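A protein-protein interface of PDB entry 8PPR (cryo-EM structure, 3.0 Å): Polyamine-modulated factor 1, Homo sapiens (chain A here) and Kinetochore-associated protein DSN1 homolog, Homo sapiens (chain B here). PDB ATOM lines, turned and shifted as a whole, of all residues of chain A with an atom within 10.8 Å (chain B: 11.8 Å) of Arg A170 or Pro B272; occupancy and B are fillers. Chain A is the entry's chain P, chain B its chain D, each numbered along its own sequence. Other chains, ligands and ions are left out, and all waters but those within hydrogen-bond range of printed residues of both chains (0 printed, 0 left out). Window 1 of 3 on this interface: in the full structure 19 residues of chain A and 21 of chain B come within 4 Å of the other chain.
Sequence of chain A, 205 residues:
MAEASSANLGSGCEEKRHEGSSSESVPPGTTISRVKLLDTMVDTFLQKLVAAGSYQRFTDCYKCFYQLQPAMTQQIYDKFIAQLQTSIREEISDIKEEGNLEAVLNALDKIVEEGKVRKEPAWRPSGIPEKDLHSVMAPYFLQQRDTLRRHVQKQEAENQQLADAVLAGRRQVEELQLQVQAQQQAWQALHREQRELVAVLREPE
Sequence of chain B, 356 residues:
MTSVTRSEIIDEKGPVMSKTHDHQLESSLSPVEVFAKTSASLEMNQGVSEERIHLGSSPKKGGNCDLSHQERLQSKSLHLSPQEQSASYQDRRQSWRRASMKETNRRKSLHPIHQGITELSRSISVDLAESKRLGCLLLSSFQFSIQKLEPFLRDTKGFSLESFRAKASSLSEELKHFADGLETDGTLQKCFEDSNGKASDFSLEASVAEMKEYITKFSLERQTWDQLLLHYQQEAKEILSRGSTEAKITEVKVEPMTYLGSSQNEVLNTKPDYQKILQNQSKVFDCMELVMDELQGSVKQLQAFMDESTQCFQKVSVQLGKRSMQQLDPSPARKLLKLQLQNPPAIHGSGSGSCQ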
ATOM      1  N   ASN A 159      19.181  -1.825 -37.622  1.00  0.00           N
ATOM      2  CA  ASN A 159      19.273  -2.245 -36.230  1.00  0.00           C
ATOM      3  C   ASN A 159      18.472  -1.329 -35.317  1.00  0.00           C
ATOM      4  O   ASN A 159      18.001  -1.768 -34.263  1.00  0.00           O
ATOM      5  CB  ASN A 159      20.737  -2.292 -35.799  1.00  0.00           C
ATOM      6  CG  ASN A 159      21.427  -3.571 -36.230  1.00  0.00           C
ATOM      7  OD1 ASN A 159      21.271  -4.021 -37.365  1.00  0.00           O
ATOM      8  ND2 ASN A 159      22.195  -4.163 -35.325  1.00  0.00           N
ATOM      9  N   LEU A 162      15.077  -2.696 -35.448  1.00  0.00           N
ATOM     10  CA  LEU A 162      15.084  -3.957 -34.712  1.00  0.00           C
ATOM     11  C   LEU A 162      15.024  -3.718 -33.205  1.00  0.00           C
ATOM     12  O   LEU A 162      14.272  -4.392 -32.489  1.00  0.00           O
ATOM     13  CB  LEU A 162      16.326  -4.761 -35.083  1.00  0.00           C
ATOM     14  CG  LEU A 162      16.356  -5.371 -36.485  1.00  0.00           C
ATOM     15  CD1 LEU A 162      17.359  -6.508 -36.542  1.00  0.00           C
ATOM     16  CD2 LEU A 162      14.971  -5.848 -36.895  1.00  0.00           C
ATOM     17  N   ALA A 163      15.804  -2.756 -32.709  1.00  0.00           N
ATOM     18  CA  ALA A 163      15.787  -2.437 -31.285  1.00  0.00           C
ATOM     19  C   ALA A 163      14.436  -1.876 -30.860  1.00  0.00           C
ATOM     20  O   ALA A 163      13.958  -2.158 -29.753  1.00  0.00           O
ATOM     21  CB  ALA A 163      16.906  -1.451 -30.956  1.00  0.00           C
ATOM     22  N   ASP A 164      13.816  -1.064 -31.717  1.00  0.00           N
ATOM     23  CA  ASP A 164      12.480  -0.561 -31.411  1.00  0.00           C
ATOM     24  C   ASP A 164      11.488  -1.707 -31.270  1.00  0.00           C
ATOM     25  O   ASP A 164      10.654  -1.718 -30.352  1.00  0.00           O
ATOM     26  CB  ASP A 164      12.032   0.409 -32.501  1.00  0.00           C
ATOM     27  CG  ASP A 164      12.847   1.687 -32.511  1.00  0.00           C
ATOM     28  OD1 ASP A 164      13.337   2.088 -31.436  1.00  0.00           O
ATOM     29  OD2 ASP A 164      13.004   2.283 -33.597  1.00  0.00           O
ATOM     30  N   ALA A 165      11.572  -2.691 -32.169  1.00  0.00           N
ATOM     31  CA  ALA A 165      10.712  -3.865 -32.066  1.00  0.00           C
ATOM     32  C   ALA A 165      10.985  -4.637 -30.781  1.00  0.00           C
ATOM     33  O   ALA A 165      10.054  -5.139 -30.138  1.00  0.00           O
ATOM     34  CB  ALA A 165      10.904  -4.765 -33.286  1.00  0.00           C
ATOM     35  N   VAL A 166      12.258  -4.746 -30.396  1.00  0.00           N
ATOM     36  CA  VAL A 166      12.604  -5.421 -29.145  1.00  0.00           C
ATOM     37  C   VAL A 166      11.951  -4.716 -27.964  1.00  0.00           C
ATOM     38  O   VAL A 166      11.393  -5.359 -27.064  1.00  0.00           O
ATOM     39  CB  VAL A 166      14.132  -5.488 -28.972  1.00  0.00           C
ATOM     40  CG1 VAL A 166      14.483  -6.004 -27.587  1.00  0.00           C
ATOM     41  CG2 VAL A 166      14.756  -6.366 -30.035  1.00  0.00           C
ATOM     42  N   LEU A 167      12.026  -3.385 -27.940  1.00  0.00           N
ATOM     43  CA  LEU A 167      11.436  -2.627 -26.842  1.00  0.00           C
ATOM     44  C   LEU A 167       9.925  -2.815 -26.793  1.00  0.00           C
ATOM     45  O   LEU A 167       9.345  -2.988 -25.712  1.00  0.00           O
ATOM     46  CB  LEU A 167      11.787  -1.148 -26.982  1.00  0.00           C
ATOM     47  CG  LEU A 167      13.267  -0.813 -26.801  1.00  0.00           C
ATOM     48  CD1 LEU A 167      13.499   0.682 -26.940  1.00  0.00           C
ATOM     49  CD2 LEU A 167      13.767  -1.320 -25.458  1.00  0.00           C
ATOM     50  N   ALA A 168       9.272  -2.783 -27.957  1.00  0.00           N
ATOM     51  CA  ALA A 168       7.829  -3.001 -27.994  1.00  0.00           C
ATOM     52  C   ALA A 168       7.470  -4.387 -27.474  1.00  0.00           C
ATOM     53  O   ALA A 168       6.507  -4.546 -26.710  1.00  0.00           O
ATOM     54  CB  ALA A 168       7.306  -2.806 -29.415  1.00  0.00           C
ATOM     55  N   GLY A 169       8.234  -5.404 -27.877  1.00  0.00           N
ATOM     56  CA  GLY A 169       7.980  -6.747 -27.386  1.00  0.00           C
ATOM     57  C   GLY A 169       8.165  -6.864 -25.887  1.00  0.00           C
ATOM     58  O   GLY A 169       7.383  -7.531 -25.205  1.00  0.00           O
ATOM     59  N   ARG A 170       9.202  -6.216 -25.352  1.00  0.00           N
ATOM     60  CA  ARG A 170       9.409  -6.227 -23.907  1.00  0.00           C
ATOM     61  C   ARG A 170       8.237  -5.579 -23.183  1.00  0.00           C
ATOM     62  O   ARG A 170       7.766  -6.091 -22.159  1.00  0.00           O
ATOM     63  CB  ARG A 170      10.713  -5.511 -23.553  1.00  0.00           C
ATOM     64  CG  ARG A 170      11.970  -6.258 -23.956  1.00  0.00           C
ATOM     65  CD  ARG A 170      13.206  -5.391 -23.777  1.00  0.00           C
ATOM     66  NE  ARG A 170      14.422  -6.075 -24.201  1.00  0.00           N
ATOM     67  CZ  ARG A 170      15.638  -5.549 -24.137  1.00  0.00           C
ATOM     68  NH1 ARG A 170      15.842  -4.337 -23.648  1.00  0.00           N
ATOM     69  NH2 ARG A 170      16.675  -6.257 -24.575  1.00  0.00           N
ATOM     70  N   ARG A 171       7.752  -4.451 -23.707  1.00  0.00           N
ATOM     71  CA  ARG A 171       6.614  -3.783 -23.086  1.00  0.00           C
ATOM     72  C   ARG A 171       5.382  -4.677 -23.099  1.00  0.00           C
ATOM     73  O   ARG A 171       4.662  -4.779 -22.095  1.00  0.00           O
ATOM     74  CB  ARG A 171       6.325  -2.466 -23.805  1.00  0.00           C
ATOM     75  CG  ARG A 171       7.313  -1.349 -23.503  1.00  0.00           C
ATOM     76  CD  ARG A 171       7.751  -1.337 -22.047  1.00  0.00           C
ATOM     77  NE  ARG A 171       8.985  -2.090 -21.847  1.00  0.00           N
ATOM     78  CZ  ARG A 171      10.198  -1.625 -22.111  1.00  0.00           C
ATOM     79  NH1 ARG A 171      10.382  -0.405 -22.587  1.00  0.00           N
ATOM     80  NH2 ARG A 171      11.252  -2.407 -21.896  1.00  0.00           N
ATOM     81  N   GLN A 172       5.127  -5.339 -24.228  1.00  0.00           N
ATOM     82  CA  GLN A 172       3.967  -6.218 -24.322  1.00  0.00           C
ATOM     83  C   GLN A 172       4.085  -7.399 -23.365  1.00  0.00           C
ATOM     84  O   GLN A 172       3.095  -7.797 -22.739  1.00  0.00           O
ATOM     85  CB  GLN A 172       3.793  -6.704 -25.758  1.00  0.00           C
ATOM     86  CG  GLN A 172       2.549  -7.542 -25.979  1.00  0.00           C
ATOM     87  CD  GLN A 172       2.252  -7.757 -27.448  1.00  0.00           C
ATOM     88  OE1 GLN A 172       3.072  -7.443 -28.311  1.00  0.00           O
ATOM     89  NE2 GLN A 172       1.077  -8.301 -27.740  1.00  0.00           N
ATOM     90  N   VAL A 173       5.282  -7.975 -23.246  1.00  0.00           N
ATOM     91  CA  VAL A 173       5.483  -9.088 -22.321  1.00  0.00           C
ATOM     92  C   VAL A 173       5.235  -8.641 -20.888  1.00  0.00           C
ATOM     93  O   VAL A 173       4.592  -9.348 -20.100  1.00  0.00           O
ATOM     94  CB  VAL A 173       6.894  -9.679 -22.493  1.00  0.00           C
ATOM     95  CG1 VAL A 173       7.206 -10.649 -21.366  1.00  0.00           C
ATOM     96  CG2 VAL A 173       7.012 -10.377 -23.837  1.00  0.00           C
ATOM     97  N   GLU A 174       5.742  -7.459 -20.527  1.00  0.00           N
ATOM     98  CA  GLU A 174       5.499  -6.934 -19.188  1.00  0.00           C
ATOM     99  C   GLU A 174       4.009  -6.747 -18.935  1.00  0.00           C
ATOM    100  O   GLU A 174       3.502  -7.098 -17.863  1.00  0.00           O
ATOM    101  CB  GLU A 174       6.240  -5.612 -19.009  1.00  0.00           C
ATOM    102  CG  GLU A 174       5.721  -4.763 -17.867  1.00  0.00           C
ATOM    103  CD  GLU A 174       6.453  -3.444 -17.749  1.00  0.00           C
ATOM    104  OE1 GLU A 174       7.657  -3.401 -18.075  1.00  0.00           O
ATOM    105  OE2 GLU A 174       5.822  -2.450 -17.333  1.00  0.00           O
ATOM    106  N   GLU A 175       3.292  -6.203 -19.920  1.00  0.00           N
ATOM    107  CA  GLU A 175       1.859  -5.983 -19.754  1.00  0.00           C
ATOM    108  C   GLU A 175       1.111  -7.300 -19.590  1.00  0.00           C
ATOM    109  O   GLU A 175       0.197  -7.408 -18.762  1.00  0.00           O
ATOM    110  CB  GLU A 175       1.317  -5.202 -20.948  1.00  0.00           C
ATOM    111  CG  GLU A 175       1.634  -3.720 -20.897  1.00  0.00           C
ATOM    112  CD  GLU A 175       1.029  -2.958 -22.056  1.00  0.00           C
ATOM    113  OE1 GLU A 175       0.054  -3.460 -22.652  1.00  0.00           O
ATOM    114  OE2 GLU A 175       1.532  -1.860 -22.372  1.00  0.00           O
ATOM    115  N   LEU A 176       1.481  -8.313 -20.375  1.00  0.00           N
ATOM    116  CA  LEU A 176       0.830  -9.615 -20.260  1.00  0.00           C
ATOM    117  C   LEU A 176       1.098 -10.245 -18.900  1.00  0.00           C
ATOM    118  O   LEU A 176       0.198 -10.840 -18.291  1.00  0.00           O
ATOM    119  CB  LEU A 176       1.303 -10.535 -21.385  1.00  0.00           C
ATOM    120  CG  LEU A 176       0.849 -10.152 -22.795  1.00  0.00           C
ATOM    121  CD1 LEU A 176       0.938 -11.341 -23.737  1.00  0.00           C
ATOM    122  CD2 LEU A 176      -0.565  -9.591 -22.774  1.00  0.00           C
ATOM    123  N   GLN A 177       2.332 -10.127 -18.407  1.00  0.00           N
ATOM    124  CA  GLN A 177       2.645 -10.643 -17.080  1.00  0.00           C
ATOM    125  C   GLN A 177       1.833  -9.924 -16.011  1.00  0.00           C
ATOM    126  O   GLN A 177       1.341 -10.552 -15.064  1.00  0.00           O
ATOM    127  CB  GLN A 177       4.141 -10.501 -16.805  1.00  0.00           C
ATOM    128  CG  GLN A 177       4.589 -11.110 -15.494  1.00  0.00           C
ATOM    129  CD  GLN A 177       6.086 -11.012 -15.297  1.00  0.00           C
ATOM    130  OE1 GLN A 177       6.795 -10.440 -16.124  1.00  0.00           O
ATOM    131  NE2 GLN A 177       6.577 -11.571 -14.197  1.00  0.00           N
ATOM    132  N   LEU A 178       1.678  -8.608 -16.151  1.00  0.00           N
ATOM    133  CA  LEU A 178       0.868  -7.855 -15.200  1.00  0.00           C
ATOM    134  C   LEU A 178      -0.588  -8.302 -15.241  1.00  0.00           C
ATOM    135  O   LEU A 178      -1.242  -8.402 -14.198  1.00  0.00           O
ATOM    136  CB  LEU A 178       0.981  -6.360 -15.492  1.00  0.00           C
ATOM    137  CG  LEU A 178       2.325  -5.738 -15.120  1.00  0.00           C
ATOM    138  CD1 LEU A 178       2.334  -4.250 -15.427  1.00  0.00           C
ATOM    139  CD2 LEU A 178       2.644  -5.993 -13.655  1.00  0.00           C
ATOM    140  N   TYR B 259      29.494  -7.824 -29.314  1.00  0.00           N
ATOM    141  CA  TYR B 259      28.433  -6.840 -29.155  1.00  0.00           C
ATOM    142  C   TYR B 259      28.855  -5.640 -28.318  1.00  0.00           C
ATOM    143  O   TYR B 259      28.061  -4.707 -28.159  1.00  0.00           O
ATOM    144  CB  TYR B 259      27.205  -7.494 -28.516  1.00  0.00           C
ATOM    145  CG  TYR B 259      26.728  -8.736 -29.231  1.00  0.00           C
ATOM    146  CD1 TYR B 259      26.162  -8.656 -30.496  1.00  0.00           C
ATOM    147  CD2 TYR B 259      26.843  -9.987 -28.641  1.00  0.00           C
ATOM    148  CE1 TYR B 259      25.723  -9.787 -31.150  1.00  0.00           C
ATOM    149  CE2 TYR B 259      26.406 -11.125 -29.291  1.00  0.00           C
ATOM    150  CZ  TYR B 259      25.846 -11.018 -30.546  1.00  0.00           C
ATOM    151  OH  TYR B 259      25.410 -12.145 -31.201  1.00  0.00           O
ATOM    152  N   SER B 263      26.178  -0.543 -31.681  1.00  0.00           N
ATOM    153  CA  SER B 263      25.385   0.652 -31.420  1.00  0.00           C
ATOM    154  C   SER B 263      24.272   0.369 -30.418  1.00  0.00           C
ATOM    155  O   SER B 263      24.036   1.164 -29.502  1.00  0.00           O
ATOM    156  CB  SER B 263      24.806   1.192 -32.727  1.00  0.00           C
ATOM    157  OG  SER B 263      23.893   0.271 -33.296  1.00  0.00           O
ATOM    158  N   GLN B 264      23.583  -0.757 -30.575  1.00  0.00           N
ATOM    159  CA  GLN B 264      22.508  -1.138 -29.659  1.00  0.00           C
ATOM    160  C   GLN B 264      23.030  -2.019 -28.530  1.00  0.00           C
ATOM    161  O   GLN B 264      22.498  -3.091 -28.245  1.00  0.00           O
ATOM    162  CB  GLN B 264      21.397  -1.837 -30.432  1.00  0.00           C
ATOM    163  CG  GLN B 264      20.932  -1.081 -31.667  1.00  0.00           C
ATOM    164  CD  GLN B 264      20.050   0.109 -31.337  1.00  0.00           C
ATOM    165  OE1 GLN B 264      19.880   0.474 -30.174  1.00  0.00           O
ATOM    166  NE2 GLN B 264      19.487   0.725 -32.368  1.00  0.00           N
ATOM    167  N   ASN B 265      24.094  -1.555 -27.873  1.00  0.00           N
ATOM    168  CA  ASN B 265      24.676  -2.322 -26.779  1.00  0.00           C
ATOM    169  C   ASN B 265      23.751  -2.346 -25.570  1.00  0.00           C
ATOM    170  O   ASN B 265      23.632  -3.374 -24.892  1.00  0.00           O
ATOM    171  CB  ASN B 265      26.039  -1.746 -26.404  1.00  0.00           C
ATOM    172  CG  ASN B 265      26.850  -2.689 -25.543  1.00  0.00           C
ATOM    173  OD1 ASN B 265      26.655  -3.903 -25.578  1.00  0.00           O
ATOM    174  ND2 ASN B 265      27.770  -2.134 -24.763  1.00  0.00           N
ATOM    175  N   GLU B 266      23.093  -1.221 -25.281  1.00  0.00           N
ATOM    176  CA  GLU B 266      22.204  -1.156 -24.126  1.00  0.00           C
ATOM    177  C   GLU B 266      21.034  -2.119 -24.271  1.00  0.00           C
ATOM    178  O   GLU B 266      20.673  -2.817 -23.317  1.00  0.00           O
ATOM    179  CB  GLU B 266      21.695   0.272 -23.940  1.00  0.00           C
ATOM    180  CG  GLU B 266      22.768   1.267 -23.549  1.00  0.00           C
ATOM    181  CD  GLU B 266      22.192   2.615 -23.167  1.00  0.00           C
ATOM    182  OE1 GLU B 266      20.955   2.719 -23.043  1.00  0.00           O
ATOM    183  OE2 GLU B 266      22.977   3.571 -22.993  1.00  0.00           O
ATOM    184  N   VAL B 267      20.431  -2.172 -25.461  1.00  0.00           N
ATOM    185  CA  VAL B 267      19.285  -3.050 -25.675  1.00  0.00           C
ATOM    186  C   VAL B 267      19.690  -4.505 -25.482  1.00  0.00           C
ATOM    187  O   VAL B 267      18.981  -5.283 -24.831  1.00  0.00           O
ATOM    188  CB  VAL B 267      18.685  -2.807 -27.071  1.00  0.00           C
ATOM    189  CG1 VAL B 267      17.724  -3.926 -27.443  1.00  0.00           C
ATOM    190  CG2 VAL B 267      17.988  -1.457 -27.121  1.00  0.00           C
ATOM    191  N   LEU B 268      20.840  -4.890 -26.035  1.00  0.00           N
ATOM    192  CA  LEU B 268      21.323  -6.255 -25.867  1.00  0.00           C
ATOM    193  C   LEU B 268      21.622  -6.558 -24.406  1.00  0.00           C
ATOM    194  O   LEU B 268      21.306  -7.647 -23.912  1.00  0.00           O
ATOM    195  CB  LEU B 268      22.572  -6.474 -26.720  1.00  0.00           C
ATOM    196  CG  LEU B 268      22.376  -6.499 -28.235  1.00  0.00           C
ATOM    197  CD1 LEU B 268      23.709  -6.298 -28.937  1.00  0.00           C
ATOM    198  CD2 LEU B 268      21.724  -7.799 -28.673  1.00  0.00           C
ATOM    199  N   ASN B 269      22.230  -5.605 -23.699  1.00  0.00           N
ATOM    200  CA  ASN B 269      22.637  -5.845 -22.320  1.00  0.00           C
ATOM    201  C   ASN B 269      21.433  -5.962 -21.396  1.00  0.00           C
ATOM    202  O   ASN B 269      21.455  -6.737 -20.433  1.00  0.00           O
ATOM    203  CB  ASN B 269      23.565  -4.725 -21.855  1.00  0.00           C
ATOM    204  CG  ASN B 269      25.024  -5.040 -22.107  1.00  0.00           C
ATOM    205  OD1 ASN B 269      25.395  -6.195 -22.312  1.00  0.00           O
ATOM    206  ND2 ASN B 269      25.861  -4.009 -22.102  1.00  0.00           N
ATOM    207  N   THR B 270      20.371  -5.205 -21.672  1.00  0.00           N
ATOM    208  CA  THR B 270      19.193  -5.154 -20.815  1.00  0.00           C
ATOM    209  C   THR B 270      18.142  -6.191 -21.189  1.00  0.00           C
ATOM    210  O   THR B 270      16.951  -5.983 -20.919  1.00  0.00           O
ATOM    211  CB  THR B 270      18.585  -3.752 -20.845  1.00  0.00           C
ATOM    212  OG1 THR B 270      18.210  -3.422 -22.188  1.00  0.00           O
ATOM    213  CG2 THR B 270      19.586  -2.728 -20.331  1.00  0.00           C
ATOM    214  N   LYS B 271      18.542  -7.293 -21.804  1.00  0.00           N
ATOM    215  CA  LYS B 271      17.573  -8.307 -22.196  1.00  0.00           C
ATOM    216  C   LYS B 271      17.042  -9.026 -20.960  1.00  0.00           C
ATOM    217  O   LYS B 271      17.831  -9.559 -20.171  1.00  0.00           O
ATOM    218  CB  LYS B 271      18.207  -9.303 -23.162  1.00  0.00           C
ATOM    219  CG  LYS B 271      17.541 -10.664 -23.172  1.00  0.00           C
ATOM    220  CD  LYS B 271      17.810 -11.388 -24.477  1.00  0.00           C
ATOM    221  CE  LYS B 271      17.313 -12.818 -24.423  1.00  0.00           C
ATOM    222  NZ  LYS B 271      17.596 -13.550 -25.688  1.00  0.00           N
ATOM    223  N   PRO B 272      15.729  -9.052 -20.750  1.00  0.00           N
ATOM    224  CA  PRO B 272      15.181  -9.713 -19.562  1.00  0.00           C
ATOM    225  C   PRO B 272      15.197 -11.227 -19.693  1.00  0.00           C
ATOM    226  O   PRO B 272      15.233 -11.791 -20.790  1.00  0.00           O
ATOM    227  CB  PRO B 272      13.747  -9.181 -19.496  1.00  0.00           C
ATOM    228  CG  PRO B 272      13.404  -8.898 -20.922  1.00  0.00           C
ATOM    229  CD  PRO B 272      14.679  -8.418 -21.566  1.00  0.00           C
ATOM    230  N   ASP B 273      15.167 -11.888 -18.538  1.00  0.00           N
ATOM    231  CA  ASP B 273      15.066 -13.340 -18.504  1.00  0.00           C
ATOM    232  C   ASP B 273      13.694 -13.785 -18.993  1.00  0.00           C
ATOM    233  O   ASP B 273      12.684 -13.119 -18.751  1.00  0.00           O
ATOM    234  CB  ASP B 273      15.313 -13.862 -17.090  1.00  0.00           C
ATOM    235  CG  ASP B 273      15.610 -15.351 -17.058  1.00  0.00           C
ATOM    236  OD1 ASP B 273      15.243 -16.063 -18.017  1.00  0.00           O
ATOM    237  OD2 ASP B 273      16.216 -15.812 -16.068  1.00  0.00           O
ATOM    238  N   TYR B 274      13.662 -14.921 -19.689  1.00  0.00           N
ATOM    239  CA  TYR B 274      12.426 -15.432 -20.261  1.00  0.00           C
ATOM    240  C   TYR B 274      12.027 -16.808 -19.751  1.00  0.00           C
ATOM    241  O   TYR B 274      10.835 -17.132 -19.786  1.00  0.00           O
ATOM    242  CB  TYR B 274      12.533 -15.476 -21.793  1.00  0.00           C
ATOM    243  CG  TYR B 274      12.601 -14.101 -22.415  1.00  0.00           C
ATOM    244  CD1 TYR B 274      11.850 -13.051 -21.904  1.00  0.00           C
ATOM    245  CD2 TYR B 274      13.426 -13.848 -23.502  1.00  0.00           C
ATOM    246  CE1 TYR B 274      11.913 -11.789 -22.464  1.00  0.00           C
ATOM    247  CE2 TYR B 274      13.495 -12.589 -24.068  1.00  0.00           C
ATOM    248  CZ  TYR B 274      12.737 -11.563 -23.546  1.00  0.00           C
ATOM    249  OH  TYR B 274      12.801 -10.308 -24.105  1.00  0.00           O
ATOM    250  N   GLN B 275      12.973 -17.620 -19.276  1.00  0.00           N
ATOM    251  CA  GLN B 275      12.622 -18.903 -18.677  1.00  0.00           C
ATOM    252  C   GLN B 275      11.957 -18.727 -17.320  1.00  0.00           C
ATOM    253  O   GLN B 275      11.084 -19.523 -16.947  1.00  0.00           O
ATOM    254  CB  GLN B 275      13.870 -19.776 -18.536  1.00  0.00           C
ATOM    255  CG  GLN B 275      13.576 -21.248 -18.304  1.00  0.00           C
ATOM    256  CD  GLN B 275      12.883 -21.901 -19.481  1.00  0.00           C
ATOM    257  OE1 GLN B 275      12.989 -21.436 -20.616  1.00  0.00           O
ATOM    258  NE2 GLN B 275      12.163 -22.984 -19.217  1.00  0.00           N
ATOM    259  N   LYS B 276      12.362 -17.697 -16.576  1.00  0.00           N
ATOM    260  CA  LYS B 276      11.757 -17.435 -15.276  1.00  0.00           C
ATOM    261  C   LYS B 276      10.264 -17.176 -15.413  1.00  0.00           C
ATOM    262  O   LYS B 276       9.477 -17.579 -14.552  1.00  0.00           O
ATOM    263  CB  LYS B 276      12.450 -16.249 -14.610  1.00  0.00           C
ATOM    264  CG  LYS B 276      13.782 -16.598 -13.977  1.00  0.00           C
ATOM    265  CD  LYS B 276      13.617 -16.921 -12.507  1.00  0.00           C
ATOM    266  CE  LYS B 276      13.258 -15.680 -11.710  1.00  0.00           C
ATOM    267  NZ  LYS B 276      12.961 -16.004 -10.289  1.00  0.00           N
ATOM    268  N   ILE B 277       9.858 -16.508 -16.492  1.00  0.00           N
ATOM    269  CA  ILE B 277       8.436 -16.281 -16.733  1.00  0.00           C
ATOM    270  C   ILE B 277       7.716 -17.606 -16.950  1.00  0.00           C
ATOM    271  O   ILE B 277       6.613 -17.829 -16.430  1.00  0.00           O
ATOM    272  CB  ILE B 277       8.251 -15.328 -17.928  1.00  0.00           C
ATOM    273  CG1 ILE B 277       8.907 -13.980 -17.632  1.00  0.00           C
ATOM    274  CG2 ILE B 277       6.777 -15.146 -18.240  1.00  0.00           C
ATOM    275  CD1 ILE B 277       8.873 -13.016 -18.796  1.00  0.00           C
ATOM    276  N   LEU B 278       8.328 -18.508 -17.721  1.00  0.00           N
ATOM    277  CA  LEU B 278       7.718 -19.811 -17.957  1.00  0.00           C
ATOM    278  C   LEU B 278       7.589 -20.608 -16.667  1.00  0.00           C
ATOM    279  O   LEU B 278       6.616 -21.349 -16.491  1.00  0.00           O
ATOM    280  CB  LEU B 278       8.536 -20.593 -18.984  1.00  0.00           C
ATOM    281  CG  LEU B 278       8.555 -20.027 -20.405  1.00  0.00           C
ATOM    282  CD1 LEU B 278       9.056 -21.070 -21.390  1.00  0.00           C
ATOM    283  CD2 LEU B 278       7.178 -19.520 -20.806  1.00  0.00           C
ATOM    284  N   ASN B 280       7.263 -19.160 -13.655  1.00  0.00           N
ATOM    285  CA  ASN B 280       6.224 -18.459 -12.917  1.00  0.00           C
ATOM    286  C   ASN B 280       4.838 -18.849 -13.404  1.00  0.00           C
ATOM    287  O   ASN B 280       3.876 -18.803 -12.634  1.00  0.00           O
ATOM    288  CB  ASN B 280       6.428 -16.950 -13.037  1.00  0.00           C
ATOM    289  CG  ASN B 280       7.684 -16.480 -12.336  1.00  0.00           C
ATOM    290  OD1 ASN B 280       8.539 -17.283 -11.966  1.00  0.00           O
ATOM    291  ND2 ASN B 280       7.806 -15.171 -12.155  1.00  0.00           N
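Ala A163 touches Gln B264 (CB to CD, 3.5 Å).
CB of Ala A163 touches CG2 of Val B267, 3.98 Å away.
Val A166 touches Val B267.
Arg A170 touches Pro B272.
Ile B277 touches Val A173.
Of the 18 printed residues of chain B, 6 touch a printed residue of chain A.
Hydrophobic or aromatic side chains of chain B that line the printed part of chain A: Val B267, Pro B272 and Ile B277.
Along chain B the printed residues that touch a printed residue of chain A span positions 264 to 277.
Hydrophobic or aromatic side chains of chain A that line the printed part of chain B: Ala A163, Val A166 and Val A173.
Among the printed residues, 9 pairs touch across the chains.
Among the printed residues, no Asp or Glu carboxylate lies within 4 Å of a Lys or Arg side-chain nitrogen of the other chain.
The backbone carbonyl oxygen of Glu B266 lies within hydrogen-bond range of the side-chain hydroxyl of Thr B270, 2.8 Å away.
The backbone carbonyl oxygen of Val B267 is in hydrogen-bond range of the side-chain hydroxyl of Thr B270, at 3.3 Å.
Leu A162 touches none of the printed residues of chain B.
Of chain B, only Val B267 (3.9 Å) comes within 4 Å of Val A166.
Ala A168 touches none of the printed residues of chain B.
No residue of chain B comes within 4 Å of Gly A169.
Arg A170 touches just these residues of chain B: Val B267 (2.5 Å), Thr B270 (2.9 Å), Lys B271 (3.3 Å) and Pro B272 (3.5 Å).
No residue of chain B comes within 4 Å of Arg A171.
Val A173 touches just one residue of chain B: Ile B277.
Leu A178 touches none of the printed residues of chain B.
Of the printed residues of chain A, Gln B264 touches Asn A159 and Ala A163.
Of the printed residues of chain A, Val B267 touches Ala A163 (3.98 Å), Val A166 (3.9 Å) and Arg A170 (2.5 Å).
Of chain A, only Arg A170 comes within 4 Å of Thr B270.
The nearest residue of chain B that does not touch Arg A170 is Tyr B274 (4.1 Å).
The nearest printed residue of chain A that does not touch Ile B277 is Gln A177 (4.3 Å).
The side-chain amide nitrogen (NE2) of Gln B264 sits at hydrogen-bond distance from the backbone carbonyl oxygen (O) of Asn A159, 3.5 Å away.
The backbone carbonyl oxygen (O) of Val B267 lies within hydrogen-bond range of the guanidinium group (NH2) of Arg A170 (2.5 Å).
NH1 of Arg A170 sits at hydrogen-bond distance from OG1 of Thr B270, 2.9 Å away.
The backbone NH of Lys B271 sits close to the guanidinium group of Arg A170 (3.5 Å).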
